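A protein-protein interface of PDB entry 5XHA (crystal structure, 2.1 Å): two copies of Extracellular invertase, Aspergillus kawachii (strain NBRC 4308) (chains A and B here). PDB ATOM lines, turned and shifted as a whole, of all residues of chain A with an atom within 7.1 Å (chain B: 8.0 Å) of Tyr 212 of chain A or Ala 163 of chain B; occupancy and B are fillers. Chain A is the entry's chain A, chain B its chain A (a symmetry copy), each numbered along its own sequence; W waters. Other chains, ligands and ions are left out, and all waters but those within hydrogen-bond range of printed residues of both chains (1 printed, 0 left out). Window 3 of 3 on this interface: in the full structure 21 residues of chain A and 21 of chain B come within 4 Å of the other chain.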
ATOM      1  N   LYS A 187       3.061 -24.360  36.971  1.00  0.00           N
ATOM      2  CA  LYS A 187       2.234 -23.292  37.506  1.00  0.00           C
ATOM      3  C   LYS A 187       0.842 -23.855  37.798  1.00  0.00           C
ATOM      4  O   LYS A 187       0.364 -24.754  37.093  1.00  0.00           O
ATOM      5  CB  LYS A 187       2.154 -22.131  36.524  1.00  0.00           C
ATOM      6  CG  LYS A 187       3.492 -21.433  36.327  1.00  0.00           C
ATOM      7  CD  LYS A 187       3.388 -20.275  35.353  1.00  0.00           C
ATOM      8  CE  LYS A 187       4.762 -19.732  35.012  1.00  0.00           C
ATOM      9  NZ  LYS A 187       4.710 -18.872  33.798  1.00  0.00           N
ATOM     10  N   THR A 190      -2.024 -25.121  35.194  1.00  0.00           N
ATOM     11  CA  THR A 190      -1.433 -25.412  33.907  1.00  0.00           C
ATOM     12  C   THR A 190      -2.362 -26.339  33.112  1.00  0.00           C
ATOM     13  O   THR A 190      -2.972 -27.253  33.660  1.00  0.00           O
ATOM     14  CB  THR A 190      -0.070 -26.104  34.102  1.00  0.00           C
ATOM     15  OG1 THR A 190       0.880 -25.145  34.578  1.00  0.00           O
ATOM     16  CG2 THR A 190       0.448 -26.711  32.812  1.00  0.00           C
ATOM     17  N   TRP A 191      -2.456 -26.078  31.816  1.00  0.00           N
ATOM     18  CA  TRP A 191      -3.143 -26.951  30.893  1.00  0.00           C
ATOM     19  C   TRP A 191      -2.157 -27.997  30.408  1.00  0.00           C
ATOM     20  O   TRP A 191      -1.043 -27.657  29.989  1.00  0.00           O
ATOM     21  CB  TRP A 191      -3.715 -26.157  29.704  1.00  0.00           C
ATOM     22  CG  TRP A 191      -4.965 -25.458  30.044  1.00  0.00           C
ATOM     23  CD1 TRP A 191      -5.115 -24.126  30.369  1.00  0.00           C
ATOM     24  CD2 TRP A 191      -6.265 -26.035  30.117  1.00  0.00           C
ATOM     25  NE1 TRP A 191      -6.436 -23.852  30.629  1.00  0.00           N
ATOM     26  CE2 TRP A 191      -7.163 -25.005  30.481  1.00  0.00           C
ATOM     27  CE3 TRP A 191      -6.769 -27.321  29.890  1.00  0.00           C
ATOM     28  CZ2 TRP A 191      -8.532 -25.227  30.637  1.00  0.00           C
ATOM     29  CZ3 TRP A 191      -8.124 -27.535  30.042  1.00  0.00           C
ATOM     30  CH2 TRP A 191      -8.993 -26.493  30.412  1.00  0.00           C
ATOM     31  N   ARG A 210       2.778 -30.101  28.445  1.00  0.00           N
ATOM     32  CA  ARG A 210       2.188 -29.022  29.224  1.00  0.00           C
ATOM     33  C   ARG A 210       2.404 -27.690  28.566  1.00  0.00           C
ATOM     34  O   ARG A 210       3.410 -27.462  27.894  1.00  0.00           O
ATOM     35  CB  ARG A 210       2.707 -28.986  30.667  1.00  0.00           C
ATOM     36  CG  ARG A 210       4.105 -28.445  30.848  1.00  0.00           C
ATOM     37  CD  ARG A 210       4.449 -28.267  32.322  1.00  0.00           C
ATOM     38  NE  ARG A 210       5.887 -28.097  32.445  1.00  0.00           N
ATOM     39  CZ  ARG A 210       6.594 -28.217  33.564  1.00  0.00           C
ATOM     40  NH1 ARG A 210       6.021 -28.526  34.722  1.00  0.00           N
ATOM     41  NH2 ARG A 210       7.905 -28.047  33.506  1.00  0.00           N
ATOM     42  N   GLN A 211       1.412 -26.831  28.755  1.00  0.00           N
ATOM     43  CA  GLN A 211       1.448 -25.428  28.373  1.00  0.00           C
ATOM     44  C   GLN A 211       2.760 -24.788  28.830  1.00  0.00           C
ATOM     45  O   GLN A 211       3.078 -24.855  30.001  1.00  0.00           O
ATOM     46  CB  GLN A 211       0.273 -24.742  29.071  1.00  0.00           C
ATOM     47  CG  GLN A 211       0.263 -23.251  29.008  1.00  0.00           C
ATOM     48  CD  GLN A 211      -0.966 -22.630  29.621  1.00  0.00           C
ATOM     49  OE1 GLN A 211      -1.337 -21.526  29.253  1.00  0.00           O
ATOM     50  NE2 GLN A 211      -1.588 -23.311  30.564  1.00  0.00           N
ATOM     51  N   TYR A 212       3.498 -24.170  27.912  1.00  0.00           N
ATOM     52  CA  TYR A 212       4.768 -23.509  28.230  1.00  0.00           C
ATOM     53  C   TYR A 212       4.603 -21.999  28.393  1.00  0.00           C
ATOM     54  O   TYR A 212       5.364 -21.365  29.113  1.00  0.00           O
ATOM     55  CB  TYR A 212       5.760 -23.779  27.104  1.00  0.00           C
ATOM     56  CG  TYR A 212       7.194 -23.358  27.359  1.00  0.00           C
ATOM     57  CD1 TYR A 212       8.027 -24.119  28.193  1.00  0.00           C
ATOM     58  CD2 TYR A 212       7.735 -22.238  26.732  1.00  0.00           C
ATOM     59  CE1 TYR A 212       9.349 -23.762  28.411  1.00  0.00           C
ATOM     60  CE2 TYR A 212       9.063 -21.875  26.938  1.00  0.00           C
ATOM     61  CZ  TYR A 212       9.858 -22.644  27.778  1.00  0.00           C
ATOM     62  OH  TYR A 212      11.167 -22.300  27.991  1.00  0.00           O
ATOM     63  N   ASP A 213       3.615 -21.436  27.700  1.00  0.00           N
ATOM     64  CA  ASP A 213       3.363 -20.009  27.688  1.00  0.00           C
ATOM     65  C   ASP A 213       1.871 -19.789  27.875  1.00  0.00           C
ATOM     66  O   ASP A 213       1.034 -20.658  27.554  1.00  0.00           O
ATOM     67  CB  ASP A 213       3.782 -19.411  26.343  1.00  0.00           C
ATOM     68  CG  ASP A 213       3.001 -20.014  25.167  1.00  0.00           C
ATOM     69  OD1 ASP A 213       3.083 -21.229  24.980  1.00  0.00           O
ATOM     70  OD2 ASP A 213       2.265 -19.297  24.470  1.00  0.00           O
ATOM     71  N   SER A 214       1.514 -18.613  28.365  1.00  0.00           N
ATOM     72  CA  SER A 214       0.108 -18.326  28.572  1.00  0.00           C
ATOM     73  C   SER A 214      -0.656 -18.166  27.257  1.00  0.00           C
ATOM     74  O   SER A 214      -1.878 -18.135  27.287  1.00  0.00           O
ATOM     75  CB  SER A 214      -0.085 -17.113  29.488  1.00  0.00           C
ATOM     76  OG  SER A 214       0.638 -15.995  29.038  1.00  0.00           O
ATOM     77  N   ASP A 215       0.035 -18.102  26.111  1.00  0.00           N
ATOM     78  CA  ASP A 215      -0.647 -17.895  24.819  1.00  0.00           C
ATOM     79  C   ASP A 215      -1.006 -19.200  24.080  1.00  0.00           C
ATOM     80  O   ASP A 215      -1.511 -19.129  22.958  1.00  0.00           O
ATOM     81  CB  ASP A 215       0.179 -16.990  23.889  1.00  0.00           C
ATOM     82  CG  ASP A 215       0.863 -15.836  24.629  1.00  0.00           C
ATOM     83  OD1 ASP A 215       1.861 -16.088  25.348  1.00  0.00           O
ATOM     84  OD2 ASP A 215       0.418 -14.672  24.480  1.00  0.00           O
ATOM     85  N   PHE A 216      -0.738 -20.360  24.703  1.00  0.00           N
ATOM     86  CA  PHE A 216      -1.036 -21.693  24.142  1.00  0.00           C
ATOM     87  C   PHE A 216      -0.255 -22.041  22.873  1.00  0.00           C
ATOM     88  O   PHE A 216      -0.603 -22.953  22.134  1.00  0.00           O
ATOM     89  CB  PHE A 216      -2.535 -21.854  23.933  1.00  0.00           C
ATOM     90  CG  PHE A 216      -3.331 -21.558  25.166  1.00  0.00           C
ATOM     91  CD1 PHE A 216      -3.228 -22.383  26.278  1.00  0.00           C
ATOM     92  CD2 PHE A 216      -4.139 -20.432  25.240  1.00  0.00           C
ATOM     93  CE1 PHE A 216      -3.939 -22.107  27.435  1.00  0.00           C
ATOM     94  CE2 PHE A 216      -4.858 -20.152  26.398  1.00  0.00           C
ATOM     95  CZ  PHE A 216      -4.760 -20.992  27.495  1.00  0.00           C
ATOM     96  N   GLN A 217       0.842 -21.326  22.671  1.00  0.00           N
ATOM     97  CA  GLN A 217       1.632 -21.405  21.460  1.00  0.00           C
ATOM     98  C   GLN A 217       2.629 -22.568  21.507  1.00  0.00           C
ATOM     99  O   GLN A 217       2.854 -23.257  20.500  1.00  0.00           O
ATOM    100  CB  GLN A 217       2.345 -20.064  21.324  1.00  0.00           C
ATOM    101  CG  GLN A 217       3.018 -19.820  20.013  1.00  0.00           C
ATOM    102  CD  GLN A 217       2.050 -19.813  18.854  1.00  0.00           C
ATOM    103  OE1 GLN A 217       0.901 -19.350  18.955  1.00  0.00           O
ATOM    104  NE2 GLN A 217       2.501 -20.355  17.755  1.00  0.00           N
ATOM    105  N   TYR A 218       3.213 -22.787  22.691  1.00  0.00           N
ATOM    106  CA  TYR A 218       4.244 -23.780  22.892  1.00  0.00           C
ATOM    107  C   TYR A 218       3.844 -24.808  23.941  1.00  0.00           C
ATOM    108  O   TYR A 218       3.250 -24.474  24.981  1.00  0.00           O
ATOM    109  CB  TYR A 218       5.581 -23.114  23.261  1.00  0.00           C
ATOM    110  CG  TYR A 218       6.106 -22.231  22.171  1.00  0.00           C
ATOM    111  CD1 TYR A 218       6.604 -22.789  20.992  1.00  0.00           C
ATOM    112  CD2 TYR A 218       6.093 -20.837  22.295  1.00  0.00           C
ATOM    113  CE1 TYR A 218       7.068 -21.996  19.965  1.00  0.00           C
ATOM    114  CE2 TYR A 218       6.556 -20.027  21.257  1.00  0.00           C
ATOM    115  CZ  TYR A 218       7.049 -20.619  20.099  1.00  0.00           C
ATOM    116  OH  TYR A 218       7.518 -19.857  19.056  1.00  0.00           O
ATOM    117  N   TRP A 219       4.164 -26.065  23.640  1.00  0.00           N
ATOM    118  CA  TRP A 219       3.732 -27.199  24.446  1.00  0.00           C
ATOM    119  C   TRP A 219       4.954 -28.037  24.774  1.00  0.00           C
ATOM    120  O   TRP A 219       5.529 -28.682  23.895  1.00  0.00           O
ATOM    121  CB  TRP A 219       2.634 -27.997  23.705  1.00  0.00           C
ATOM    122  CG  TRP A 219       1.413 -27.173  23.598  1.00  0.00           C
ATOM    123  CD1 TRP A 219       1.143 -26.256  22.640  1.00  0.00           C
ATOM    124  CD2 TRP A 219       0.337 -27.104  24.540  1.00  0.00           C
ATOM    125  NE1 TRP A 219      -0.056 -25.631  22.906  1.00  0.00           N
ATOM    126  CE2 TRP A 219      -0.560 -26.123  24.080  1.00  0.00           C
ATOM    127  CE3 TRP A 219       0.048 -27.774  25.732  1.00  0.00           C
ATOM    128  CZ2 TRP A 219      -1.732 -25.810  24.752  1.00  0.00           C
ATOM    129  CZ3 TRP A 219      -1.106 -27.457  26.407  1.00  0.00           C
ATOM    130  CH2 TRP A 219      -1.991 -26.488  25.917  1.00  0.00           C
ATOM    131  N   GLU A 220       5.365 -27.994  26.044  1.00  0.00           N
ATOM    132  CA  GLU A 220       6.574 -28.676  26.483  1.00  0.00           C
ATOM    133  C   GLU A 220       6.301 -30.175  26.586  1.00  0.00           C
ATOM    134  O   GLU A 220       5.382 -30.587  27.269  1.00  0.00           O
ATOM    135  CB  GLU A 220       7.011 -28.104  27.828  1.00  0.00           C
ATOM    136  CG  GLU A 220       8.306 -28.667  28.371  1.00  0.00           C
ATOM    137  CD  GLU A 220       8.669 -28.057  29.715  1.00  0.00           C
ATOM    138  OE1 GLU A 220       7.851 -27.357  30.338  1.00  0.00           O
ATOM    139  OE2 GLU A 220       9.793 -28.278  30.144  1.00  0.00           O
ATOM    140  N   ARG B 131       4.309 -18.047  13.299  1.00  0.00           N
ATOM    141  CA  ARG B 131       4.706 -19.413  13.571  1.00  0.00           C
ATOM    142  C   ARG B 131       4.523 -20.287  12.311  1.00  0.00           C
ATOM    143  O   ARG B 131       3.510 -20.178  11.611  1.00  0.00           O
ATOM    144  CB  ARG B 131       3.882 -19.944  14.754  1.00  0.00           C
ATOM    145  CG  ARG B 131       4.244 -21.351  15.220  1.00  0.00           C
ATOM    146  CD  ARG B 131       5.436 -21.370  16.173  1.00  0.00           C
ATOM    147  NE  ARG B 131       5.734 -22.747  16.585  1.00  0.00           N
ATOM    148  CZ  ARG B 131       5.108 -23.407  17.551  1.00  0.00           C
ATOM    149  NH1 ARG B 131       4.134 -22.823  18.238  1.00  0.00           N
ATOM    150  NH2 ARG B 131       5.441 -24.667  17.831  1.00  0.00           N
ATOM    151  N   PRO B 160      11.830 -24.047  13.879  1.00  0.00           N
ATOM    152  CA  PRO B 160      13.014 -23.808  14.689  1.00  0.00           C
ATOM    153  C   PRO B 160      12.963 -24.578  16.009  1.00  0.00           C
ATOM    154  O   PRO B 160      11.938 -25.137  16.346  1.00  0.00           O
ATOM    155  CB  PRO B 160      12.979 -22.293  14.937  1.00  0.00           C
ATOM    156  CG  PRO B 160      11.566 -21.887  14.728  1.00  0.00           C
ATOM    157  CD  PRO B 160      10.945 -22.869  13.804  1.00  0.00           C
ATOM    158  N   PRO B 161      14.077 -24.624  16.747  1.00  0.00           N
ATOM    159  CA  PRO B 161      14.046 -25.320  18.034  1.00  0.00           C
ATOM    160  C   PRO B 161      12.952 -24.773  18.951  1.00  0.00           C
ATOM    161  O   PRO B 161      12.487 -23.629  18.782  1.00  0.00           O
ATOM    162  CB  PRO B 161      15.434 -25.047  18.623  1.00  0.00           C
ATOM    163  CG  PRO B 161      16.304 -24.750  17.446  1.00  0.00           C
ATOM    164  CD  PRO B 161      15.419 -24.125  16.406  1.00  0.00           C
ATOM    165  N   PHE B 162      12.541 -25.608  19.898  1.00  0.00           N
ATOM    166  CA  PHE B 162      11.390 -25.353  20.745  1.00  0.00           C
ATOM    167  C   PHE B 162      11.398 -23.954  21.363  1.00  0.00           C
ATOM    168  O   PHE B 162      12.363 -23.560  22.018  1.00  0.00           O
ATOM    169  CB  PHE B 162      11.329 -26.415  21.851  1.00  0.00           C
ATOM    170  CG  PHE B 162      10.216 -26.194  22.841  1.00  0.00           C
ATOM    171  CD1 PHE B 162       8.900 -26.491  22.499  1.00  0.00           C
ATOM    172  CD2 PHE B 162      10.477 -25.674  24.096  1.00  0.00           C
ATOM    173  CE1 PHE B 162       7.868 -26.284  23.397  1.00  0.00           C
ATOM    174  CE2 PHE B 162       9.446 -25.456  25.002  1.00  0.00           C
ATOM    175  CZ  PHE B 162       8.145 -25.764  24.652  1.00  0.00           C
ATOM    176  N   ALA B 163      10.305 -23.225  21.161  1.00  0.00           N
ATOM    177  CA  ALA B 163      10.095 -21.895  21.733  1.00  0.00           C
ATOM    178  C   ALA B 163      11.083 -20.813  21.288  1.00  0.00           C
ATOM    179  O   ALA B 163      11.081 -19.736  21.870  1.00  0.00           O
ATOM    180  CB  ALA B 163      10.037 -21.960  23.255  1.00  0.00           C
ATOM    181  N   TYR B 164      11.900 -21.061  20.260  1.00  0.00           N
ATOM    182  CA  TYR B 164      12.813 -20.007  19.774  1.00  0.00           C
ATOM    183  C   TYR B 164      12.022 -18.950  19.020  1.00  0.00           C
ATOM    184  O   TYR B 164      11.268 -19.282  18.122  1.00  0.00           O
ATOM    185  CB  TYR B 164      13.876 -20.575  18.835  1.00  0.00           C
ATOM    186  CG  TYR B 164      15.083 -21.207  19.496  1.00  0.00           C
ATOM    187  CD1 TYR B 164      14.992 -21.824  20.743  1.00  0.00           C
ATOM    188  CD2 TYR B 164      16.314 -21.247  18.837  1.00  0.00           C
ATOM    189  CE1 TYR B 164      16.091 -22.425  21.325  1.00  0.00           C
ATOM    190  CE2 TYR B 164      17.417 -21.850  19.411  1.00  0.00           C
ATOM    191  CZ  TYR B 164      17.298 -22.433  20.654  1.00  0.00           C
ATOM    192  OH  TYR B 164      18.376 -23.044  21.251  1.00  0.00           O
ATOM    193  N   ASN B 165      12.193 -17.687  19.389  1.00  0.00           N
ATOM    194  CA  ASN B 165      11.500 -16.572  18.759  1.00  0.00           C
ATOM    195  C   ASN B 165      12.403 -16.039  17.637  1.00  0.00           C
ATOM    196  O   ASN B 165      13.112 -15.033  17.792  1.00  0.00           O
ATOM    197  CB  ASN B 165      11.223 -15.508  19.828  1.00  0.00           C
ATOM    198  CG  ASN B 165      10.412 -14.329  19.314  1.00  0.00           C
ATOM    199  OD1 ASN B 165       9.831 -14.352  18.237  1.00  0.00           O
ATOM    200  ND2 ASN B 165      10.372 -13.283  20.109  1.00  0.00           N
ATOM    201  N   VAL B 166      12.403 -16.751  16.515  1.00  0.00           N
ATOM    202  CA  VAL B 166      13.279 -16.426  15.400  1.00  0.00           C
ATOM    203  C   VAL B 166      12.830 -15.164  14.650  1.00  0.00           C
ATOM    204  O   VAL B 166      11.641 -14.885  14.546  1.00  0.00           O
ATOM    205  CB  VAL B 166      13.356 -17.589  14.382  1.00  0.00           C
ATOM    206  CG1 VAL B 166      13.970 -18.830  14.997  1.00  0.00           C
ATOM    207  CG2 VAL B 166      11.975 -17.902  13.820  1.00  0.00           C
ATOM    208  N   LEU B 199      17.477 -14.476  16.344  1.00  0.00           N
ATOM    209  CA  LEU B 199      16.450 -14.467  17.390  1.00  0.00           C
ATOM    210  C   LEU B 199      16.133 -13.032  17.807  1.00  0.00           C
ATOM    211  O   LEU B 199      17.029 -12.220  17.968  1.00  0.00           O
ATOM    212  CB  LEU B 199      16.932 -15.263  18.605  1.00  0.00           C
ATOM    213  CG  LEU B 199      17.220 -16.733  18.356  1.00  0.00           C
ATOM    214  CD1 LEU B 199      17.862 -17.354  19.592  1.00  0.00           C
ATOM    215  CD2 LEU B 199      15.934 -17.457  18.005  1.00  0.00           C
HETATM  216  O   HOH W   1       9.248 -21.052  17.521  1.00  0.00           O
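Among the printed residues, pairs that only touch across the chains: Tyr 212 of chain A with Phe 162 of chain B (3.7 Å), Tyr 212 of chain A with Ala 163 of chain B (3.8 Å), Tyr 218 of chain A with Arg 131 of chain B (3.4 Å), Tyr 218 of chain A with Phe 162 of chain B (3.9 Å), Tyr 218 of chain A with Ala 163 of chain B (3.5 Å), Tyr 218 of chain A with Tyr 164 of chain B (3.9 Å), Trp 219 of chain A with Phe 162 of chain B (3.4 Å) and Glu 220 of chain A with Phe 162 of chain B (3.8 Å).
The side-chain carboxylate of Glu 220 of chain A lies within salt-bridge range of the guanidinium group of Arg 210 of chain A, at 3.0 Å.
The backbone NH of Tyr 218 of chain A is in hydrogen-bond range of the side-chain carboxylate of Asp 213 of chain A, 2.8 Å away.
O of Phe 216 of chain A is in hydrogen-bond range of NE1 of Trp 219 of chain A (2.8 Å).
The backbone NH (N) of Tyr 212 of chain A is in hydrogen-bond range of the backbone carbonyl oxygen (O) of Tyr 218 of chain A (3.0 Å).
OD2 of Asp 213 of chain A is in hydrogen-bond range of N of Gln 217 of chain A, at 3.1 Å.
O of Gln 217 of chain A is in hydrogen-bond range of NH1 of Arg 131 of chain B, at 2.6 Å.
Lys 187 of chain A touches none of the printed residues of chain B.
Thr 190 of chain A touches none of the printed residues of chain B.
Printed residues of chain B within 4 Å of Tyr 212 of chain A: Phe 162 and Ala 163.
Printed residues of chain B within 4 Å of Tyr 218 of chain A: Arg 131 (3.4 Å), Phe 162 (3.9 Å), Ala 163 (3.5 Å) and Tyr 164 (3.9 Å).
Of the printed residues of chain B, Glu 220 of chain A touches Phe 162.
Printed residues of chain A within 4 Å of Phe 162 of chain B: Tyr 212 (3.7 Å), Tyr 218 (3.9 Å), Trp 219 (3.4 Å) and Glu 220 (3.8 Å).
Of the printed residues of chain A, Tyr 164 of chain B touches Tyr 218 (3.9 Å).
The nearest printed residue of chain A that does not touch Ala 163 of chain B is Trp 219 of chain A (7.2 Å).
Hydrophobic or aromatic side chains of chain B that line the printed part of chain A: Phe 162 and Ala 163.
Along chain B the printed residues that touch a printed residue of chain A span positions 131 to 164.
Hydrophobic or aromatic side chains of chain A within 4 Å of the printed part of chain B: Tyr 212 and Tyr 218.
Among the printed residues, 9 pairs touch across the chains.
Among the printed residues, no Asp or Glu carboxylate lies within 4 Å of a Lys or Arg side-chain nitrogen of the other chain.
No position is printed for both chains.
Of the 9 pairs that touch across the chains among the printed residues, none has its exchanged pair printed and touching as well.
Water W1 bridges the side-chain hydroxyl (OH) of Tyr 218 of chain A and the backbone carbonyl oxygen (O) of Tyr 164 of chain B.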
